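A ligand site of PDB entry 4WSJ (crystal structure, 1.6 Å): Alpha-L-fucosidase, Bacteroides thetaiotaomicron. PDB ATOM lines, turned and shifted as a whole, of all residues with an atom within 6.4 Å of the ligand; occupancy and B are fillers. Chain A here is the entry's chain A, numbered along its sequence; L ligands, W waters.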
ATOM      1  N   PHE A  30      -8.339 -23.210  11.879  1.00  0.00           N
ATOM      2  CA  PHE A  30      -9.577 -22.721  11.240  1.00  0.00           C
ATOM      3  C   PHE A  30      -9.190 -21.548  10.390  1.00  0.00           C
ATOM      4  O   PHE A  30      -8.374 -20.676  10.798  1.00  0.00           O
ATOM      5  CB  PHE A  30     -10.669 -22.294  12.259  1.00  0.00           C
ATOM      6  CG  PHE A  30     -12.055 -22.862  11.961  1.00  0.00           C
ATOM      7  CD1 PHE A  30     -12.725 -22.501  10.787  1.00  0.00           C
ATOM      8  CD2 PHE A  30     -12.716 -23.623  12.937  1.00  0.00           C
ATOM      9  CE1 PHE A  30     -13.977 -23.001  10.540  1.00  0.00           C
ATOM     10  CE2 PHE A  30     -13.996 -24.177  12.653  1.00  0.00           C
ATOM     11  CZ  PHE A  30     -14.623 -23.831  11.442  1.00  0.00           C
ATOM     12  N   HIS A  32     -11.288 -18.436   8.613  1.00  0.00           N
ATOM     13  CA  HIS A  32     -12.503 -17.665   8.366  1.00  0.00           C
ATOM     14  C   HIS A  32     -12.139 -16.552   7.389  1.00  0.00           C
ATOM     15  O   HIS A  32     -11.426 -15.617   7.738  1.00  0.00           O
ATOM     16  CB  HIS A  32     -13.105 -17.033   9.635  1.00  0.00           C
ATOM     17  CG  HIS A  32     -14.040 -17.915  10.346  1.00  0.00           C
ATOM     18  ND1 HIS A  32     -13.600 -18.969  11.138  1.00  0.00           N
ATOM     19  CD2 HIS A  32     -15.403 -17.913  10.459  1.00  0.00           C
ATOM     20  CE1 HIS A  32     -14.656 -19.569  11.671  1.00  0.00           C
ATOM     21  NE2 HIS A  32     -15.748 -18.954  11.251  1.00  0.00           N
ATOM     22  N   ALA A  51     -18.197  -9.530  16.554  1.00  0.00           N
ATOM     23  CA  ALA A  51     -17.406 -10.364  15.651  1.00  0.00           C
ATOM     24  C   ALA A  51     -17.459  -9.771  14.199  1.00  0.00           C
ATOM     25  O   ALA A  51     -18.561  -9.528  13.665  1.00  0.00           O
ATOM     26  CB  ALA A  51     -17.906 -11.752  15.677  1.00  0.00           C
ATOM     27  N   GLU A  53     -17.032 -10.988  11.267  1.00  0.00           N
ATOM     28  CA  GLU A  53     -17.764 -11.735  10.262  1.00  0.00           C
ATOM     29  C   GLU A  53     -19.271 -11.555  10.315  1.00  0.00           C
ATOM     30  O   GLU A  53     -19.995 -11.904   9.341  1.00  0.00           O
ATOM     31  CB  GLU A  53     -17.348 -13.227  10.251  1.00  0.00           C
ATOM     32  CG  GLU A  53     -17.793 -14.114  11.408  1.00  0.00           C
ATOM     33  CD  GLU A  53     -17.182 -13.857  12.775  1.00  0.00           C
ATOM     34  OE1 GLU A  53     -16.199 -13.115  12.920  1.00  0.00           O
ATOM     35  OE2 GLU A  53     -17.788 -14.489  13.705  1.00  0.00           O
ATOM     36  N   TRP A  54     -19.757 -10.944  11.420  1.00  0.00           N
ATOM     37  CA  TRP A  54     -21.147 -10.584  11.586  1.00  0.00           C
ATOM     38  C   TRP A  54     -21.424  -9.090  11.303  1.00  0.00           C
ATOM     39  O   TRP A  54     -22.537  -8.635  11.576  1.00  0.00           O
ATOM     40  CB  TRP A  54     -21.623 -10.945  13.005  1.00  0.00           C
ATOM     41  CG  TRP A  54     -22.017 -12.383  13.201  1.00  0.00           C
ATOM     42  CD1 TRP A  54     -21.146 -13.481  13.354  1.00  0.00           C
ATOM     43  CD2 TRP A  54     -23.321 -12.919  13.336  1.00  0.00           C
ATOM     44  NE1 TRP A  54     -21.874 -14.625  13.512  1.00  0.00           N
ATOM     45  CE2 TRP A  54     -23.219 -14.302  13.512  1.00  0.00           C
ATOM     46  CE3 TRP A  54     -24.642 -12.332  13.328  1.00  0.00           C
ATOM     47  CZ2 TRP A  54     -24.325 -15.115  13.688  1.00  0.00           C
ATOM     48  CZ3 TRP A  54     -25.731 -13.174  13.456  1.00  0.00           C
ATOM     49  CH2 TRP A  54     -25.581 -14.540  13.654  1.00  0.00           C
ATOM     50  N   THR A  98     -13.797 -21.891   5.870  1.00  0.00           N
ATOM     51  CA  THR A  98     -15.145 -21.372   5.555  1.00  0.00           C
ATOM     52  C   THR A  98     -15.390 -21.421   4.030  1.00  0.00           C
ATOM     53  O   THR A  98     -14.916 -20.532   3.296  1.00  0.00           O
ATOM     54  CB  THR A  98     -15.333 -19.927   6.012  1.00  0.00           C
ATOM     55  OG1 THR A  98     -14.265 -19.083   5.562  1.00  0.00           O
ATOM     56  CG2 THR A  98     -15.353 -19.833   7.520  1.00  0.00           C
ATOM     57  N   HIS A 101     -19.871 -18.503   4.428  1.00  0.00           N
ATOM     58  CA  HIS A 101     -20.321 -18.022   5.756  1.00  0.00           C
ATOM     59  C   HIS A 101     -21.764 -17.480   5.625  1.00  0.00           C
ATOM     60  O   HIS A 101     -22.421 -17.660   4.602  1.00  0.00           O
ATOM     61  CB  HIS A 101     -19.316 -16.996   6.313  1.00  0.00           C
ATOM     62  CG  HIS A 101     -19.284 -16.975   7.829  1.00  0.00           C
ATOM     63  ND1 HIS A 101     -20.147 -16.195   8.583  1.00  0.00           N
ATOM     64  CD2 HIS A 101     -18.585 -17.715   8.721  1.00  0.00           C
ATOM     65  CE1 HIS A 101     -19.920 -16.399   9.874  1.00  0.00           C
ATOM     66  NE2 HIS A 101     -19.004 -17.350   9.979  1.00  0.00           N
ATOM     67  N   HIS A 102     -22.284 -16.869   6.689  1.00  0.00           N
ATOM     68  CA  HIS A 102     -23.695 -16.468   6.690  1.00  0.00           C
ATOM     69  C   HIS A 102     -23.944 -15.506   5.533  1.00  0.00           C
ATOM     70  O   HIS A 102     -25.063 -15.501   5.016  1.00  0.00           O
ATOM     71  CB  HIS A 102     -24.060 -15.790   8.028  1.00  0.00           C
ATOM     72  CG  HIS A 102     -23.678 -16.603   9.251  1.00  0.00           C
ATOM     73  ND1 HIS A 102     -23.844 -17.975   9.303  1.00  0.00           N
ATOM     74  CD2 HIS A 102     -23.263 -16.215  10.488  1.00  0.00           C
ATOM     75  CE1 HIS A 102     -23.477 -18.407  10.517  1.00  0.00           C
ATOM     76  NE2 HIS A 102     -23.114 -17.363  11.252  1.00  0.00           N
ATOM     77  N   TYR A 144     -16.118 -25.943   6.534  1.00  0.00           N
ATOM     78  CA  TYR A 144     -17.172 -25.168   7.268  1.00  0.00           C
ATOM     79  C   TYR A 144     -18.228 -24.792   6.214  1.00  0.00           C
ATOM     80  O   TYR A 144     -17.895 -24.364   5.095  1.00  0.00           O
ATOM     81  CB  TYR A 144     -16.556 -23.917   7.870  1.00  0.00           C
ATOM     82  CG  TYR A 144     -17.552 -22.892   8.378  1.00  0.00           C
ATOM     83  CD1 TYR A 144     -18.345 -22.169   7.493  1.00  0.00           C
ATOM     84  CD2 TYR A 144     -17.651 -22.613   9.758  1.00  0.00           C
ATOM     85  CE1 TYR A 144     -19.308 -21.245   7.949  1.00  0.00           C
ATOM     86  CE2 TYR A 144     -18.552 -21.654  10.215  1.00  0.00           C
ATOM     87  CZ  TYR A 144     -19.347 -20.990   9.324  1.00  0.00           C
ATOM     88  OH  TYR A 144     -20.345 -20.106   9.813  1.00  0.00           O
ATOM     89  N   MET A 148     -27.744 -21.238   7.230  1.00  0.00           N
ATOM     90  CA  MET A 148     -28.204 -19.829   7.114  1.00  0.00           C
ATOM     91  C   MET A 148     -27.458 -19.075   6.052  1.00  0.00           C
ATOM     92  O   MET A 148     -26.244 -19.037   6.019  1.00  0.00           O
ATOM     93  CB  MET A 148     -28.170 -19.088   8.467  1.00  0.00           C
ATOM     94  CG  MET A 148     -28.657 -17.631   8.407  1.00  0.00           C
ATOM     95  SD  MET A 148     -28.783 -16.916  10.055  1.00  0.00           S
ATOM     96  CE  MET A 148     -27.022 -16.653  10.384  1.00  0.00           C
ATOM     97  N   TRP A 193     -18.475 -29.232   8.605  1.00  0.00           N
ATOM     98  CA  TRP A 193     -18.693 -28.612   9.924  1.00  0.00           C
ATOM     99  C   TRP A 193     -19.718 -27.503   9.712  1.00  0.00           C
ATOM    100  O   TRP A 193     -19.458 -26.478   9.108  1.00  0.00           O
ATOM    101  CB  TRP A 193     -17.368 -28.021  10.448  1.00  0.00           C
ATOM    102  CG  TRP A 193     -17.328 -27.601  11.895  1.00  0.00           C
ATOM    103  CD1 TRP A 193     -16.912 -28.389  12.947  1.00  0.00           C
ATOM    104  CD2 TRP A 193     -17.760 -26.357  12.486  1.00  0.00           C
ATOM    105  NE1 TRP A 193     -16.982 -27.703  14.109  1.00  0.00           N
ATOM    106  CE2 TRP A 193     -17.483 -26.445  13.861  1.00  0.00           C
ATOM    107  CE3 TRP A 193     -18.291 -25.165  11.981  1.00  0.00           C
ATOM    108  CZ2 TRP A 193     -17.739 -25.420  14.737  1.00  0.00           C
ATOM    109  CZ3 TRP A 193     -18.516 -24.133  12.868  1.00  0.00           C
ATOM    110  CH2 TRP A 193     -18.281 -24.269  14.215  1.00  0.00           C
ATOM    111  N   PHE A 194     -20.957 -27.791  10.123  1.00  0.00           N
ATOM    112  CA  PHE A 194     -22.074 -26.887   9.861  1.00  0.00           C
ATOM    113  C   PHE A 194     -22.225 -25.828  10.951  1.00  0.00           C
ATOM    114  O   PHE A 194     -21.960 -26.057  12.125  1.00  0.00           O
ATOM    115  CB  PHE A 194     -23.341 -27.714   9.759  1.00  0.00           C
ATOM    116  CG  PHE A 194     -23.393 -28.547   8.492  1.00  0.00           C
ATOM    117  CD1 PHE A 194     -23.901 -28.005   7.313  1.00  0.00           C
ATOM    118  CD2 PHE A 194     -22.919 -29.835   8.479  1.00  0.00           C
ATOM    119  CE1 PHE A 194     -23.929 -28.739   6.110  1.00  0.00           C
ATOM    120  CE2 PHE A 194     -22.976 -30.581   7.306  1.00  0.00           C
ATOM    121  CZ  PHE A 194     -23.466 -30.007   6.126  1.00  0.00           C
ATOM    122  N   ASP A 195     -22.655 -24.653  10.523  1.00  0.00           N
ATOM    123  CA  ASP A 195     -23.021 -23.553  11.378  1.00  0.00           C
ATOM    124  C   ASP A 195     -24.268 -22.882  10.765  1.00  0.00           C
ATOM    125  O   ASP A 195     -24.704 -23.234   9.665  1.00  0.00           O
ATOM    126  CB  ASP A 195     -21.858 -22.601  11.466  1.00  0.00           C
ATOM    127  CG  ASP A 195     -21.924 -21.613  12.645  1.00  0.00           C
ATOM    128  OD1 ASP A 195     -22.884 -21.545  13.476  1.00  0.00           O
ATOM    129  OD2 ASP A 195     -20.877 -20.760  12.735  1.00  0.00           O
ATOM    130  N   GLY A 196     -24.872 -21.928  11.478  1.00  0.00           N
ATOM    131  CA  GLY A 196     -26.138 -21.309  11.029  1.00  0.00           C
ATOM    132  C   GLY A 196     -27.278 -22.303  10.955  1.00  0.00           C
ATOM    133  O   GLY A 196     -28.078 -22.269   9.989  1.00  0.00           O
ATOM    134  N   TRP A 198     -29.255 -23.096  13.957  1.00  0.00           N
ATOM    135  CA  TRP A 198     -30.014 -22.944  15.203  1.00  0.00           C
ATOM    136  C   TRP A 198     -31.455 -22.487  15.008  1.00  0.00           C
ATOM    137  O   TRP A 198     -32.273 -22.573  15.918  1.00  0.00           O
ATOM    138  CB  TRP A 198     -29.286 -21.941  16.140  1.00  0.00           C
ATOM    139  CG  TRP A 198     -29.139 -20.629  15.489  1.00  0.00           C
ATOM    140  CD1 TRP A 198     -30.115 -19.671  15.320  1.00  0.00           C
ATOM    141  CD2 TRP A 198     -27.945 -20.071  14.915  1.00  0.00           C
ATOM    142  NE1 TRP A 198     -29.633 -18.611  14.654  1.00  0.00           N
ATOM    143  CE2 TRP A 198     -28.302 -18.821  14.364  1.00  0.00           C
ATOM    144  CE3 TRP A 198     -26.635 -20.515  14.812  1.00  0.00           C
ATOM    145  CZ2 TRP A 198     -27.364 -17.986  13.737  1.00  0.00           C
ATOM    146  CZ3 TRP A 198     -25.718 -19.704  14.175  1.00  0.00           C
ATOM    147  CH2 TRP A 198     -26.071 -18.462  13.635  1.00  0.00           C
ATOM    148  N   ARG A 228     -23.443 -30.136  15.332  1.00  0.00           N
ATOM    149  CA  ARG A 228     -24.162 -28.836  15.211  1.00  0.00           C
ATOM    150  C   ARG A 228     -25.149 -28.832  14.068  1.00  0.00           C
ATOM    151  O   ARG A 228     -26.049 -28.034  14.065  1.00  0.00           O
ATOM    152  CB  ARG A 228     -23.153 -27.686  15.167  1.00  0.00           C
ATOM    153  CG  ARG A 228     -23.627 -26.272  14.940  1.00  0.00           C
ATOM    154  CD  ARG A 228     -22.532 -25.302  15.254  1.00  0.00           C
ATOM    155  NE  ARG A 228     -22.402 -25.128  16.724  1.00  0.00           N
ATOM    156  CZ  ARG A 228     -21.272 -24.950  17.409  1.00  0.00           C
ATOM    157  NH1 ARG A 228     -20.102 -25.070  16.853  1.00  0.00           N
ATOM    158  NH2 ARG A 228     -21.338 -24.728  18.725  1.00  0.00           N
ATOM    159  N   GLU A 254     -16.758 -23.413  22.219  1.00  0.00           N
ATOM    160  CA  GLU A 254     -16.054 -22.242  21.766  1.00  0.00           C
ATOM    161  C   GLU A 254     -15.755 -21.252  22.893  1.00  0.00           C
ATOM    162  O   GLU A 254     -14.723 -20.618  22.838  1.00  0.00           O
ATOM    163  CB  GLU A 254     -16.848 -21.515  20.700  1.00  0.00           C
ATOM    164  CG  GLU A 254     -17.016 -22.222  19.388  1.00  0.00           C
ATOM    165  CD  GLU A 254     -18.057 -23.334  19.317  1.00  0.00           C
ATOM    166  OE1 GLU A 254     -18.911 -23.478  20.189  1.00  0.00           O
ATOM    167  OE2 GLU A 254     -17.977 -24.142  18.367  1.00  0.00           O
ATOM    168  N   CYS A 274     -13.268 -25.344  18.949  1.00  0.00           N
ATOM    169  CA  CYS A 274     -12.672 -24.404  18.056  1.00  0.00           C
ATOM    170  C   CYS A 274     -12.529 -23.087  18.830  1.00  0.00           C
ATOM    171  O   CYS A 274     -13.405 -22.737  19.605  1.00  0.00           O
ATOM    172  CB  CYS A 274     -13.503 -24.184  16.824  1.00  0.00           C
ATOM    173  SG  CYS A 274     -13.755 -25.694  15.858  1.00  0.00           S
ATOM    174  N   ASN A 280     -13.673 -12.869  20.737  1.00  0.00           N
ATOM    175  CA  ASN A 280     -14.699 -13.355  19.838  1.00  0.00           C
ATOM    176  C   ASN A 280     -14.572 -12.676  18.480  1.00  0.00           C
ATOM    177  O   ASN A 280     -15.392 -11.809  18.155  1.00  0.00           O
ATOM    178  CB  ASN A 280     -16.114 -13.143  20.385  1.00  0.00           C
ATOM    179  CG  ASN A 280     -17.211 -13.727  19.470  1.00  0.00           C
ATOM    180  OD1 ASN A 280     -16.991 -14.627  18.673  1.00  0.00           O
ATOM    181  ND2 ASN A 280     -18.438 -13.250  19.676  1.00  0.00           N
ATOM    182  N   TRP A 282     -13.727 -14.075  14.628  1.00  0.00           N
ATOM    183  CA  TRP A 282     -13.371 -15.196  13.734  1.00  0.00           C
ATOM    184  C   TRP A 282     -12.820 -14.704  12.400  1.00  0.00           C
ATOM    185  O   TRP A 282     -11.708 -15.013  11.986  1.00  0.00           O
ATOM    186  CB  TRP A 282     -14.508 -16.154  13.557  1.00  0.00           C
ATOM    187  CG  TRP A 282     -15.020 -16.777  14.852  1.00  0.00           C
ATOM    188  CD1 TRP A 282     -15.943 -16.262  15.703  1.00  0.00           C
ATOM    189  CD2 TRP A 282     -14.665 -18.066  15.366  1.00  0.00           C
ATOM    190  NE1 TRP A 282     -16.177 -17.135  16.749  1.00  0.00           N
ATOM    191  CE2 TRP A 282     -15.398 -18.248  16.567  1.00  0.00           C
ATOM    192  CE3 TRP A 282     -13.744 -19.040  14.991  1.00  0.00           C
ATOM    193  CZ2 TRP A 282     -15.264 -19.390  17.370  1.00  0.00           C
ATOM    194  CZ3 TRP A 282     -13.628 -20.169  15.792  1.00  0.00           C
ATOM    195  CH2 TRP A 282     -14.452 -20.373  16.930  1.00  0.00           C
HETATM  196  C1  LIG L   1     -17.141 -20.636  14.287  1.00  0.00           C
HETATM  197  C2  LIG L   1     -18.275 -19.627  14.588  1.00  0.00           C
HETATM  198  C3  LIG L   1     -18.319 -18.458  13.567  1.00  0.00           C
HETATM  199  O1  LIG L   1     -18.316 -19.019  12.193  1.00  0.00           O
HETATM  200  C4  LIG L   1     -19.581 -17.692  13.750  1.00  0.00           C
HETATM  201  O2  LIG L   1     -19.455 -16.422  13.021  1.00  0.00           O
HETATM  202  C5  LIG L   1     -20.691 -18.466  13.310  1.00  0.00           C
HETATM  203  O3  LIG L   1     -21.966 -17.719  13.714  1.00  0.00           O
HETATM  204  C6  LIG L   1     -20.798 -19.849  13.827  1.00  0.00           C
HETATM  205  C7  LIG L   1     -19.597 -20.358  14.717  1.00  0.00           C
HETATM  206  N1  LIG L   1     -19.964 -20.277  16.168  1.00  0.00           N
HETATM  207  C8  LIG L   1     -20.739 -21.218  16.671  1.00  0.00           C
HETATM  208  O4  LIG L   1     -21.283 -22.145  16.039  1.00  0.00           O
HETATM  209  C9  LIG L   1     -21.045 -21.020  18.157  1.00  0.00           C
HETATM  210  O   HOH W   1     -19.500 -17.547  17.478  1.00  0.00           O
HETATM  211  O   HOH W   2     -22.853 -17.501  16.204  1.00  0.00           O
HETATM  212  O   HOH W   3     -24.023 -22.238  16.272  1.00  0.00           O
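The side-chain carboxylate (OD2) of Asp 195 is covalently linked to a carbon (C6) of the ligand, 1.4 Å away.
NE1 of Trp 54 is in hydrogen-bond range of O2 of the ligand (3.1 Å).
NH1 of Arg 228 lies close to O4 of the ligand (3.3 Å).
NE2 of His 32 lies within hydrogen-bond range of O1 of the ligand (2.7 Å).
A ring nitrogen (NE2) of His 101 sits at hydrogen-bond distance from an oxygen (O1) of the ligand, 2.9 Å away.
The side-chain carboxylate (OE2) of Glu 53 is in hydrogen-bond range of an oxygen (O2) of the ligand.
A ring nitrogen (NE2) of His 102 is in hydrogen-bond range of an oxygen (O3) of the ligand (2.7 Å).
OH of Tyr 144 lies close to O1 of the ligand, at 3.3 Å.
OE1 of Glu 53 is in hydrogen-bond range of N of Trp 282 (3.2 Å).
OE2 of Glu 254 lies within salt-bridge range of NH1 of Arg 228.
OD1 of Asn 280 is in hydrogen-bond range of NE1 of Trp 282, 3.3 Å away.
OD2 of Asp 195 sits at hydrogen-bond distance from OH of Tyr 144 (3.0 Å).
NE2 of His 101 sits at hydrogen-bond distance from OH of Tyr 144 (3.1 Å).
Residues that only touch the ligand: Trp 282 (3.7 Å), Trp 193 (3.8 Å) and Glu 254 (3.8 Å).
11 residues have an atom within 4 Å of the ligand: His 32, Glu 53, Trp 54, His 101, His 102, Tyr 144, Trp 193, Asp 195, Arg 228, Glu 254 and Trp 282.
The nearest printed residue that does not touch the ligand is Trp 198 (4.2 Å).
Water W3 lies within hydrogen-bond range of O4 of the ligand (2.8 Å), OD1 of Asp 195 (3.1 Å) and NE of Arg 228 (3.3 Å).
Water W1 bridges a nitrogen (N1) of the ligand and the indole nitrogen (NE1) of Trp 282.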
